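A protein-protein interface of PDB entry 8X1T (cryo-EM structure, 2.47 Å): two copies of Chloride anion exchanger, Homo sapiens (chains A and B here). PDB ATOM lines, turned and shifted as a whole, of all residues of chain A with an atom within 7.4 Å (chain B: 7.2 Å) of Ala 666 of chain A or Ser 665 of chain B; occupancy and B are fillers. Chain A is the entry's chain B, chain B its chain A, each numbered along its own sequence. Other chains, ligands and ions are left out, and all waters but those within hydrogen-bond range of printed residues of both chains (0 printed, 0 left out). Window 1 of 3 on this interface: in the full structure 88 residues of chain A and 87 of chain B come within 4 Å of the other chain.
Of chain B, only Ser 665 (3.8 Å) and Ser 668 (3.0 Å) come within 4 Å of Ala 666 of chain A. Ser 665 of chain B touches two residues of chain A. Of the printed residues of chain B, Ser 665 of chain A touches Ser 665 and Ala 666. Of the printed residues of chain A, Pro 554 of chain B touches Ser 668 (3.4 Å). Phe 664 of chain A touches none of the printed residues of chain B. Cys 551 of chain B touches none of the printed residues of chain A. The nearest residue of chain B that does not touch Ala 666 of chain A is Ala 666 of chain B (4.02 Å). The nearest printed residue of chain A that does not touch Pro 552 of chain B is Phe 669 of chain A (5.7 Å).
Pro 552 of chain A touches Ser 668 of chain B, and with the chains exchanged Ser 668 of chain A touches Pro 552 of chain B. Ser 665 of chain A touches its own counterpart, Ser 665 of chain B. Ser 665 of chain A touches Ala 666 of chain B, and with the chains exchanged Ala 666 of chain A touches Ser 665 of chain B. Ser 668 of chain B touches its own counterpart, Ser 668 of chain A. 14 positions are printed for both chains. Of the 13 pairs that touch across the chains among the printed residues, 12 have their exchanged pair printed and touching as well.
NH1 of Arg 550 of chain A is in salt-bridge range of OD1 of Asp 698 of chain B, 3.5 Å away. The side-chain hydroxyl (OG) of Ser 668 of chain B is in hydrogen-bond range of the backbone carbonyl oxygen (O) of Ala 666 of chain A (3.0 Å). The backbone carbonyl oxygen of Ala 666 of chain B is in hydrogen-bond range of the side-chain hydroxyl of Ser 668 of chain A (3.1 Å).
Among the printed residues, pairs that only touch across the chains: Pro 552 of chain A with Ser 668 of chain B (3.7 Å), Ser 553 of chain A with Ser 668 of chain B (3.4 Å), Pro 554 of chain A with Ser 668 of chain B (3.2 Å), Ser 665 of chain A with Ser 665 of chain B (3.9 Å), Ser 665 of chain A with Ala 666 of chain B (3.2 Å), Ala 666 of chain A with Ser 665 of chain B (3.8 Å), Ser 668 of chain A with Pro 552 of chain B (3.5 Å), Ser 668 of chain A with Ser 553 of chain B (3.7 Å), Ser 668 of chain A with Pro 554 of chain B (3.4 Å) and Ser 668 of chain A with Ser 668 of chain B (3.7 Å).
The side-chain carboxylate of Asp 663 of chain A is in salt-bridge range of the guanidinium group of Arg 550 of chain A, at 3.0 Å. The guanidinium group (NH2) of Arg 550 of chain A lies within hydrogen-bond range of the side-chain hydroxyl (OG) of Ser 665 of chain A (3.0 Å). SG of Cys 551 of chain B sits at hydrogen-bond distance from OG of Ser 553 of chain B (3.6 Å). OG of Ser 665 of chain B is in hydrogen-bond range of NH2 of Arg 550 of chain B (3.1 Å).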
ATOM      1  N   ARG A 550     -11.825 -11.951  -5.667  1.00  0.00           N
ATOM      2  CA  ARG A 550     -10.878 -11.873  -6.768  1.00  0.00           C
ATOM      3  C   ARG A 550     -11.630 -11.858  -8.090  1.00  0.00           C
ATOM      4  O   ARG A 550     -12.416 -12.763  -8.369  1.00  0.00           O
ATOM      5  CB  ARG A 550      -9.905 -13.049  -6.719  1.00  0.00           C
ATOM      6  CG  ARG A 550      -8.999 -13.132  -7.917  1.00  0.00           C
ATOM      7  CD  ARG A 550      -8.140 -14.370  -7.878  1.00  0.00           C
ATOM      8  NE  ARG A 550      -7.556 -14.644  -9.183  1.00  0.00           N
ATOM      9  CZ  ARG A 550      -6.412 -14.125  -9.611  1.00  0.00           C
ATOM     10  NH1 ARG A 550      -5.956 -14.431 -10.814  1.00  0.00           N
ATOM     11  NH2 ARG A 550      -5.725 -13.303  -8.837  1.00  0.00           N
ATOM     12  N   CYS A 551     -11.402 -10.817  -8.887  1.00  0.00           N
ATOM     13  CA  CYS A 551     -11.821 -10.788 -10.281  1.00  0.00           C
ATOM     14  C   CYS A 551     -10.590 -10.977 -11.151  1.00  0.00           C
ATOM     15  O   CYS A 551      -9.686 -10.129 -11.119  1.00  0.00           O
ATOM     16  CB  CYS A 551     -12.522  -9.477 -10.624  1.00  0.00           C
ATOM     17  SG  CYS A 551     -13.115  -9.371 -12.328  1.00  0.00           S
ATOM     18  N   PRO A 552     -10.506 -12.114 -11.849  1.00  0.00           N
ATOM     19  CA  PRO A 552      -9.355 -12.536 -12.644  1.00  0.00           C
ATOM     20  C   PRO A 552      -9.158 -11.929 -14.014  1.00  0.00           C
ATOM     21  O   PRO A 552      -8.704 -12.645 -14.895  1.00  0.00           O
ATOM     22  CB  PRO A 552      -9.586 -14.032 -12.787  1.00  0.00           C
ATOM     23  CG  PRO A 552     -11.059 -14.169 -12.788  1.00  0.00           C
ATOM     24  CD  PRO A 552     -11.596 -13.096 -11.901  1.00  0.00           C
ATOM     25  N   SER A 553      -9.603 -10.686 -14.203  1.00  0.00           N
ATOM     26  CA  SER A 553      -9.543 -10.036 -15.503  1.00  0.00           C
ATOM     27  C   SER A 553      -9.564  -8.529 -15.400  1.00  0.00           C
ATOM     28  O   SER A 553      -9.873  -7.986 -14.348  1.00  0.00           O
ATOM     29  CB  SER A 553     -10.756 -10.449 -16.337  1.00  0.00           C
ATOM     30  OG  SER A 553     -11.925  -9.762 -15.933  1.00  0.00           O
ATOM     31  N   PRO A 554      -9.237  -7.838 -16.500  1.00  0.00           N
ATOM     32  CA  PRO A 554      -9.376  -6.380 -16.473  1.00  0.00           C
ATOM     33  C   PRO A 554     -10.842  -6.003 -16.299  1.00  0.00           C
ATOM     34  O   PRO A 554     -11.709  -6.688 -16.818  1.00  0.00           O
ATOM     35  CB  PRO A 554      -8.907  -5.957 -17.864  1.00  0.00           C
ATOM     36  CG  PRO A 554      -8.060  -7.083 -18.347  1.00  0.00           C
ATOM     37  CD  PRO A 554      -8.668  -8.320 -17.767  1.00  0.00           C
ATOM     38  N   ILE A 555     -11.116  -4.926 -15.586  1.00  0.00           N
ATOM     39  CA  ILE A 555     -12.487  -4.500 -15.386  1.00  0.00           C
ATOM     40  C   ILE A 555     -12.734  -3.268 -16.214  1.00  0.00           C
ATOM     41  O   ILE A 555     -11.977  -2.309 -16.139  1.00  0.00           O
ATOM     42  CB  ILE A 555     -12.801  -4.243 -13.903  1.00  0.00           C
ATOM     43  CG1 ILE A 555     -12.379  -5.450 -13.063  1.00  0.00           C
ATOM     44  CG2 ILE A 555     -14.280  -3.944 -13.719  1.00  0.00           C
ATOM     45  CD1 ILE A 555     -12.604  -5.273 -11.580  1.00  0.00           C
ATOM     46  N   ASP A 663      -8.818  -8.562  -4.403  1.00  0.00           N
ATOM     47  CA  ASP A 663      -7.545  -9.016  -4.958  1.00  0.00           C
ATOM     48  C   ASP A 663      -7.463  -8.566  -6.409  1.00  0.00           C
ATOM     49  O   ASP A 663      -7.918  -9.260  -7.318  1.00  0.00           O
ATOM     50  CB  ASP A 663      -7.414 -10.525  -4.833  1.00  0.00           C
ATOM     51  CG  ASP A 663      -6.138 -11.047  -5.449  1.00  0.00           C
ATOM     52  OD1 ASP A 663      -5.098 -10.372  -5.324  1.00  0.00           O
ATOM     53  OD2 ASP A 663      -6.169 -12.138  -6.054  1.00  0.00           O
ATOM     54  N   PHE A 664      -6.838  -7.429  -6.652  1.00  0.00           N
ATOM     55  CA  PHE A 664      -6.734  -6.873  -7.994  1.00  0.00           C
ATOM     56  C   PHE A 664      -5.474  -7.196  -8.779  1.00  0.00           C
ATOM     57  O   PHE A 664      -5.115  -6.468  -9.669  1.00  0.00           O
ATOM     58  CB  PHE A 664      -6.873  -5.360  -7.913  1.00  0.00           C
ATOM     59  CG  PHE A 664      -8.278  -4.878  -8.009  1.00  0.00           C
ATOM     60  CD1 PHE A 664      -9.313  -5.671  -7.596  1.00  0.00           C
ATOM     61  CD2 PHE A 664      -8.561  -3.621  -8.499  1.00  0.00           C
ATOM     62  CE1 PHE A 664     -10.609  -5.243  -7.683  1.00  0.00           C
ATOM     63  CE2 PHE A 664      -9.861  -3.174  -8.581  1.00  0.00           C
ATOM     64  CZ  PHE A 664     -10.889  -3.991  -8.169  1.00  0.00           C
ATOM     65  N   SER A 665      -4.811  -8.288  -8.456  1.00  0.00           N
ATOM     66  CA  SER A 665      -3.601  -8.663  -9.146  1.00  0.00           C
ATOM     67  C   SER A 665      -3.806  -8.929 -10.635  1.00  0.00           C
ATOM     68  O   SER A 665      -3.032  -8.488 -11.442  1.00  0.00           O
ATOM     69  CB  SER A 665      -2.960  -9.858  -8.474  1.00  0.00           C
ATOM     70  OG  SER A 665      -3.777 -10.983  -8.595  1.00  0.00           O
ATOM     71  N   ALA A 666      -4.889  -9.596 -10.978  1.00  0.00           N
ATOM     72  CA  ALA A 666      -5.226  -9.917 -12.343  1.00  0.00           C
ATOM     73  C   ALA A 666      -6.016  -8.822 -13.043  1.00  0.00           C
ATOM     74  O   ALA A 666      -6.391  -8.976 -14.173  1.00  0.00           O
ATOM     75  CB  ALA A 666      -5.974 -11.232 -12.393  1.00  0.00           C
ATOM     76  N   VAL A 667      -6.257  -7.711 -12.373  1.00  0.00           N
ATOM     77  CA  VAL A 667      -6.980  -6.601 -12.989  1.00  0.00           C
ATOM     78  C   VAL A 667      -5.932  -5.717 -13.660  1.00  0.00           C
ATOM     79  O   VAL A 667      -5.266  -4.915 -13.008  1.00  0.00           O
ATOM     80  CB  VAL A 667      -7.818  -5.823 -11.972  1.00  0.00           C
ATOM     81  CG1 VAL A 667      -8.428  -4.596 -12.613  1.00  0.00           C
ATOM     82  CG2 VAL A 667      -8.902  -6.707 -11.402  1.00  0.00           C
ATOM     83  N   SER A 668      -5.782  -5.873 -14.974  1.00  0.00           N
ATOM     84  CA  SER A 668      -4.719  -5.191 -15.700  1.00  0.00           C
ATOM     85  C   SER A 668      -4.996  -3.698 -15.828  1.00  0.00           C
ATOM     86  O   SER A 668      -4.122  -2.869 -15.563  1.00  0.00           O
ATOM     87  CB  SER A 668      -4.541  -5.824 -17.079  1.00  0.00           C
ATOM     88  OG  SER A 668      -4.533  -7.236 -16.981  1.00  0.00           O
ATOM     89  N   PHE A 669      -6.204  -3.335 -16.242  1.00  0.00           N
ATOM     90  CA  PHE A 669      -6.556  -1.940 -16.440  1.00  0.00           C
ATOM     91  C   PHE A 669      -7.987  -1.690 -15.990  1.00  0.00           C
ATOM     92  O   PHE A 669      -8.768  -2.616 -15.761  1.00  0.00           O
ATOM     93  CB  PHE A 669      -6.370  -1.510 -17.906  1.00  0.00           C
ATOM     94  CG  PHE A 669      -7.227  -2.263 -18.890  1.00  0.00           C
ATOM     95  CD1 PHE A 669      -8.539  -1.892 -19.122  1.00  0.00           C
ATOM     96  CD2 PHE A 669      -6.704  -3.318 -19.610  1.00  0.00           C
ATOM     97  CE1 PHE A 669      -9.317  -2.570 -20.027  1.00  0.00           C
ATOM     98  CE2 PHE A 669      -7.479  -3.996 -20.520  1.00  0.00           C
ATOM     99  CZ  PHE A 669      -8.786  -3.620 -20.729  1.00  0.00           C
ATOM    100  N   VAL A 695      -5.675  -4.960  -2.905  1.00  0.00           N
ATOM    101  CA  VAL A 695      -4.357  -5.551  -2.746  1.00  0.00           C
ATOM    102  C   VAL A 695      -3.895  -6.121  -4.080  1.00  0.00           C
ATOM    103  O   VAL A 695      -4.688  -6.361  -4.991  1.00  0.00           O
ATOM    104  CB  VAL A 695      -4.354  -6.643  -1.661  1.00  0.00           C
ATOM    105  CG1 VAL A 695      -4.854  -6.084  -0.348  1.00  0.00           C
ATOM    106  CG2 VAL A 695      -5.217  -7.795  -2.090  1.00  0.00           C
ATOM    107  N   GLY A 696      -2.587  -6.331  -4.184  1.00  0.00           N
ATOM    108  CA  GLY A 696      -2.012  -6.982  -5.343  1.00  0.00           C
ATOM    109  C   GLY A 696      -1.710  -6.085  -6.519  1.00  0.00           C
ATOM    110  O   GLY A 696      -1.274  -6.587  -7.558  1.00  0.00           O
ATOM    111  N   THR A 697      -1.915  -4.780  -6.390  1.00  0.00           N
ATOM    112  CA  THR A 697      -1.718  -3.849  -7.488  1.00  0.00           C
ATOM    113  C   THR A 697      -0.299  -3.298  -7.485  1.00  0.00           C
ATOM    114  O   THR A 697       0.316  -3.117  -6.432  1.00  0.00           O
ATOM    115  CB  THR A 697      -2.712  -2.695  -7.394  1.00  0.00           C
ATOM    116  OG1 THR A 697      -2.724  -2.187  -6.056  1.00  0.00           O
ATOM    117  CG2 THR A 697      -4.090  -3.167  -7.746  1.00  0.00           C
ATOM    118  N   PHE A 701      -0.623   1.066 -11.404  1.00  0.00           N
ATOM    119  CA  PHE A 701      -2.070   1.004 -11.239  1.00  0.00           C
ATOM    120  C   PHE A 701      -2.573   2.144 -10.363  1.00  0.00           C
ATOM    121  O   PHE A 701      -3.539   2.831 -10.707  1.00  0.00           O
ATOM    122  CB  PHE A 701      -2.453  -0.351 -10.643  1.00  0.00           C
ATOM    123  CG  PHE A 701      -3.918  -0.662 -10.715  1.00  0.00           C
ATOM    124  CD1 PHE A 701      -4.762  -0.322  -9.672  1.00  0.00           C
ATOM    125  CD2 PHE A 701      -4.452  -1.310 -11.812  1.00  0.00           C
ATOM    126  CE1 PHE A 701      -6.097  -0.613  -9.730  1.00  0.00           C
ATOM    127  CE2 PHE A 701      -5.792  -1.602 -11.871  1.00  0.00           C
ATOM    128  CZ  PHE A 701      -6.613  -1.254 -10.831  1.00  0.00           C
ATOM    129  N   ARG B 550       7.991  -8.993 -15.877  1.00  0.00           N
ATOM    130  CA  ARG B 550       6.566  -8.820 -15.632  1.00  0.00           C
ATOM    131  C   ARG B 550       5.918  -8.137 -16.827  1.00  0.00           C
ATOM    132  O   ARG B 550       6.351  -7.057 -17.242  1.00  0.00           O
ATOM    133  CB  ARG B 550       6.328  -8.007 -14.362  1.00  0.00           C
ATOM    134  CG  ARG B 550       4.986  -7.324 -14.325  1.00  0.00           C
ATOM    135  CD  ARG B 550       4.729  -6.668 -12.989  1.00  0.00           C
ATOM    136  NE  ARG B 550       3.359  -6.184 -12.885  1.00  0.00           N
ATOM    137  CZ  ARG B 550       2.365  -6.884 -12.356  1.00  0.00           C
ATOM    138  NH1 ARG B 550       1.145  -6.373 -12.305  1.00  0.00           N
ATOM    139  NH2 ARG B 550       2.590  -8.097 -11.882  1.00  0.00           N
ATOM    140  N   CYS B 551       4.891  -8.778 -17.385  1.00  0.00           N
ATOM    141  CA  CYS B 551       3.992  -8.164 -18.350  1.00  0.00           C
ATOM    142  C   CYS B 551       2.660  -7.912 -17.663  1.00  0.00           C
ATOM    143  O   CYS B 551       2.010  -8.872 -17.224  1.00  0.00           O
ATOM    144  CB  CYS B 551       3.801  -9.057 -19.572  1.00  0.00           C
ATOM    145  SG  CYS B 551       2.712  -8.364 -20.834  1.00  0.00           S
ATOM    146  N   PRO B 552       2.226  -6.662 -17.518  1.00  0.00           N
ATOM    147  CA  PRO B 552       1.030  -6.349 -16.730  1.00  0.00           C
ATOM    148  C   PRO B 552      -0.263  -6.339 -17.538  1.00  0.00           C
ATOM    149  O   PRO B 552      -1.080  -5.420 -17.423  1.00  0.00           O
ATOM    150  CB  PRO B 552       1.353  -4.957 -16.188  1.00  0.00           C
ATOM    151  CG  PRO B 552       2.123  -4.334 -17.310  1.00  0.00           C
ATOM    152  CD  PRO B 552       2.879  -5.439 -18.011  1.00  0.00           C
ATOM    153  N   SER B 553      -0.411  -7.332 -18.408  1.00  0.00           N
ATOM    154  CA  SER B 553      -1.596  -7.425 -19.256  1.00  0.00           C
ATOM    155  C   SER B 553      -1.808  -8.831 -19.789  1.00  0.00           C
ATOM    156  O   SER B 553      -0.892  -9.642 -19.786  1.00  0.00           O
ATOM    157  CB  SER B 553      -1.489  -6.460 -20.439  1.00  0.00           C
ATOM    158  OG  SER B 553      -0.532  -6.905 -21.377  1.00  0.00           O
ATOM    159  N   PRO B 554      -3.029  -9.129 -20.245  1.00  0.00           N
ATOM    160  CA  PRO B 554      -3.248 -10.433 -20.872  1.00  0.00           C
ATOM    161  C   PRO B 554      -2.446 -10.522 -22.157  1.00  0.00           C
ATOM    162  O   PRO B 554      -2.326  -9.532 -22.865  1.00  0.00           O
ATOM    163  CB  PRO B 554      -4.740 -10.427 -21.194  1.00  0.00           C
ATOM    164  CG  PRO B 554      -5.330  -9.363 -20.335  1.00  0.00           C
ATOM    165  CD  PRO B 554      -4.261  -8.331 -20.169  1.00  0.00           C
ATOM    166  N   LEU B 662       9.005 -15.462 -14.776  1.00  0.00           N
ATOM    167  CA  LEU B 662       8.003 -14.691 -15.499  1.00  0.00           C
ATOM    168  C   LEU B 662       6.828 -14.445 -14.563  1.00  0.00           C
ATOM    169  O   LEU B 662       6.104 -15.379 -14.210  1.00  0.00           O
ATOM    170  CB  LEU B 662       7.553 -15.420 -16.762  1.00  0.00           C
ATOM    171  CG  LEU B 662       8.598 -15.709 -17.835  1.00  0.00           C
ATOM    172  CD1 LEU B 662       8.032 -16.674 -18.843  1.00  0.00           C
ATOM    173  CD2 LEU B 662       9.037 -14.436 -18.520  1.00  0.00           C
ATOM    174  N   ASP B 663       6.640 -13.191 -14.165  1.00  0.00           N
ATOM    175  CA  ASP B 663       5.566 -12.814 -13.250  1.00  0.00           C
ATOM    176  C   ASP B 663       4.270 -12.715 -14.044  1.00  0.00           C
ATOM    177  O   ASP B 663       3.916 -11.651 -14.554  1.00  0.00           O
ATOM    178  CB  ASP B 663       5.898 -11.503 -12.551  1.00  0.00           C
ATOM    179  CG  ASP B 663       4.809 -11.054 -11.607  1.00  0.00           C
ATOM    180  OD1 ASP B 663       4.115 -11.923 -11.042  1.00  0.00           O
ATOM    181  OD2 ASP B 663       4.651  -9.831 -11.418  1.00  0.00           O
ATOM    182  N   PHE B 664       3.548 -13.831 -14.141  1.00  0.00           N
ATOM    183  CA  PHE B 664       2.312 -13.921 -14.907  1.00  0.00           C
ATOM    184  C   PHE B 664       1.088 -13.623 -14.054  1.00  0.00           C
ATOM    185  O   PHE B 664       0.000 -14.130 -14.334  1.00  0.00           O
ATOM    186  CB  PHE B 664       2.187 -15.306 -15.540  1.00  0.00           C
ATOM    187  CG  PHE B 664       2.688 -15.383 -16.951  1.00  0.00           C
ATOM    188  CD1 PHE B 664       3.774 -14.638 -17.361  1.00  0.00           C
ATOM    189  CD2 PHE B 664       2.072 -16.212 -17.866  1.00  0.00           C
ATOM    190  CE1 PHE B 664       4.228 -14.716 -18.655  1.00  0.00           C
ATOM    191  CE2 PHE B 664       2.526 -16.290 -19.157  1.00  0.00           C
ATOM    192  CZ  PHE B 664       3.605 -15.543 -19.551  1.00  0.00           C
ATOM    193  N   SER B 665       1.248 -12.802 -13.016  1.00  0.00           N
ATOM    194  CA  SER B 665       0.157 -12.559 -12.079  1.00  0.00           C
ATOM    195  C   SER B 665      -0.953 -11.730 -12.708  1.00  0.00           C
ATOM    196  O   SER B 665      -2.135 -12.062 -12.567  1.00  0.00           O
ATOM    197  CB  SER B 665       0.691 -11.875 -10.828  1.00  0.00           C
ATOM    198  OG  SER B 665       0.788 -10.478 -11.024  1.00  0.00           O
ATOM    199  N   ALA B 666      -0.599 -10.652 -13.400  1.00  0.00           N
ATOM    200  CA  ALA B 666      -1.582  -9.788 -14.037  1.00  0.00           C
ATOM    201  C   ALA B 666      -1.925 -10.220 -15.450  1.00  0.00           C
ATOM    202  O   ALA B 666      -2.687  -9.526 -16.124  1.00  0.00           O
ATOM    203  CB  ALA B 666      -1.089  -8.340 -14.055  1.00  0.00           C
ATOM    204  N   VAL B 667      -1.380 -11.340 -15.918  1.00  0.00           N
ATOM    205  CA  VAL B 667      -1.712 -11.873 -17.237  1.00  0.00           C
ATOM    206  C   VAL B 667      -3.028 -12.629 -17.091  1.00  0.00           C
ATOM    207  O   VAL B 667      -3.077 -13.715 -16.518  1.00  0.00           O
ATOM    208  CB  VAL B 667      -0.602 -12.762 -17.795  1.00  0.00           C
ATOM    209  CG1 VAL B 667      -1.069 -13.442 -19.052  1.00  0.00           C
ATOM    210  CG2 VAL B 667       0.634 -11.939 -18.072  1.00  0.00           C
ATOM    211  N   SER B 668      -4.104 -12.045 -17.614  1.00  0.00           N
ATOM    212  CA  SER B 668      -5.441 -12.588 -17.410  1.00  0.00           C
ATOM    213  C   SER B 668      -5.665 -13.855 -18.230  1.00  0.00           C
ATOM    214  O   SER B 668      -5.926 -14.926 -17.677  1.00  0.00           O
ATOM    215  CB  SER B 668      -6.484 -11.531 -17.757  1.00  0.00           C
ATOM    216  OG  SER B 668      -6.431 -10.463 -16.831  1.00  0.00           O
ATOM    217  N   ILE B 694       7.125 -19.769 -14.302  1.00  0.00           N
ATOM    218  CA  ILE B 694       5.960 -18.919 -14.421  1.00  0.00           C
ATOM    219  C   ILE B 694       5.325 -18.886 -13.055  1.00  0.00           C
ATOM    220  O   ILE B 694       5.045 -19.925 -12.473  1.00  0.00           O
ATOM    221  CB  ILE B 694       4.973 -19.432 -15.475  1.00  0.00           C
ATOM    222  CG1 ILE B 694       5.681 -19.596 -16.820  1.00  0.00           C
ATOM    223  CG2 ILE B 694       3.790 -18.485 -15.596  1.00  0.00           C
ATOM    224  CD1 ILE B 694       4.794 -20.137 -17.915  1.00  0.00           C
ATOM    225  N   VAL B 695       5.112 -17.695 -12.526  1.00  0.00           N
ATOM    226  CA  VAL B 695       4.595 -17.579 -11.176  1.00  0.00           C
ATOM    227  C   VAL B 695       3.429 -16.628 -11.080  1.00  0.00           C
ATOM    228  O   VAL B 695       3.115 -15.922 -12.034  1.00  0.00           O
ATOM    229  CB  VAL B 695       5.692 -17.072 -10.216  1.00  0.00           C
ATOM    230  CG1 VAL B 695       6.881 -18.020 -10.211  1.00  0.00           C
ATOM    231  CG2 VAL B 695       6.126 -15.666 -10.601  1.00  0.00           C
ATOM    232  N   GLY B 696       2.789 -16.604  -9.921  1.00  0.00           N
ATOM    233  CA  GLY B 696       1.704 -15.676  -9.698  1.00  0.00           C
ATOM    234  C   GLY B 696       0.390 -16.030 -10.349  1.00  0.00           C
ATOM    235  O   GLY B 696      -0.546 -15.227 -10.284  1.00  0.00           O
ATOM    236  N   THR B 697       0.289 -17.166 -11.022  1.00  0.00           N
ATOM    237  CA  THR B 697      -0.937 -17.498 -11.753  1.00  0.00           C
ATOM    238  C   THR B 697      -1.955 -18.255 -10.910  1.00  0.00           C
ATOM    239  O   THR B 697      -1.595 -18.879  -9.920  1.00  0.00           O
ATOM    240  CB  THR B 697      -0.633 -18.344 -13.006  1.00  0.00           C
ATOM    241  OG1 THR B 697      -0.029 -19.582 -12.616  1.00  0.00           O
ATOM    242  CG2 THR B 697       0.305 -17.602 -13.937  1.00  0.00           C
ATOM    243  N   ASP B 698      -3.229 -18.200 -11.293  1.00  0.00           N
ATOM    244  CA  ASP B 698      -4.256 -18.967 -10.572  1.00  0.00           C
ATOM    245  C   ASP B 698      -4.467 -20.353 -11.171  1.00  0.00           C
ATOM    246  O   ASP B 698      -3.942 -20.654 -12.238  1.00  0.00           O
ATOM    247  CB  ASP B 698      -5.583 -18.203 -10.484  1.00  0.00           C
ATOM    248  CG  ASP B 698      -6.237 -17.995 -11.833  1.00  0.00           C
ATOM    249  OD1 ASP B 698      -7.369 -17.468 -11.866  1.00  0.00           O
ATOM    250  OD2 ASP B 698      -5.630 -18.350 -12.861  1.00  0.00           O
ATOM    251  N   ILE B 724       6.844 -15.284  -6.808  1.00  0.00           N
ATOM    252  CA  ILE B 724       8.210 -14.995  -7.232  1.00  0.00           C
ATOM    253  C   ILE B 724       9.223 -15.458  -6.196  1.00  0.00           C
ATOM    254  O   ILE B 724      10.230 -16.058  -6.542  1.00  0.00           O
ATOM    255  CB  ILE B 724       8.409 -13.485  -7.510  1.00  0.00           C
ATOM    256  CG1 ILE B 724       7.522 -13.039  -8.672  1.00  0.00           C
ATOM    257  CG2 ILE B 724       9.870 -13.170  -7.796  1.00  0.00           C
ATOM    258  CD1 ILE B 724       7.499 -11.544  -8.888  1.00  0.00           C
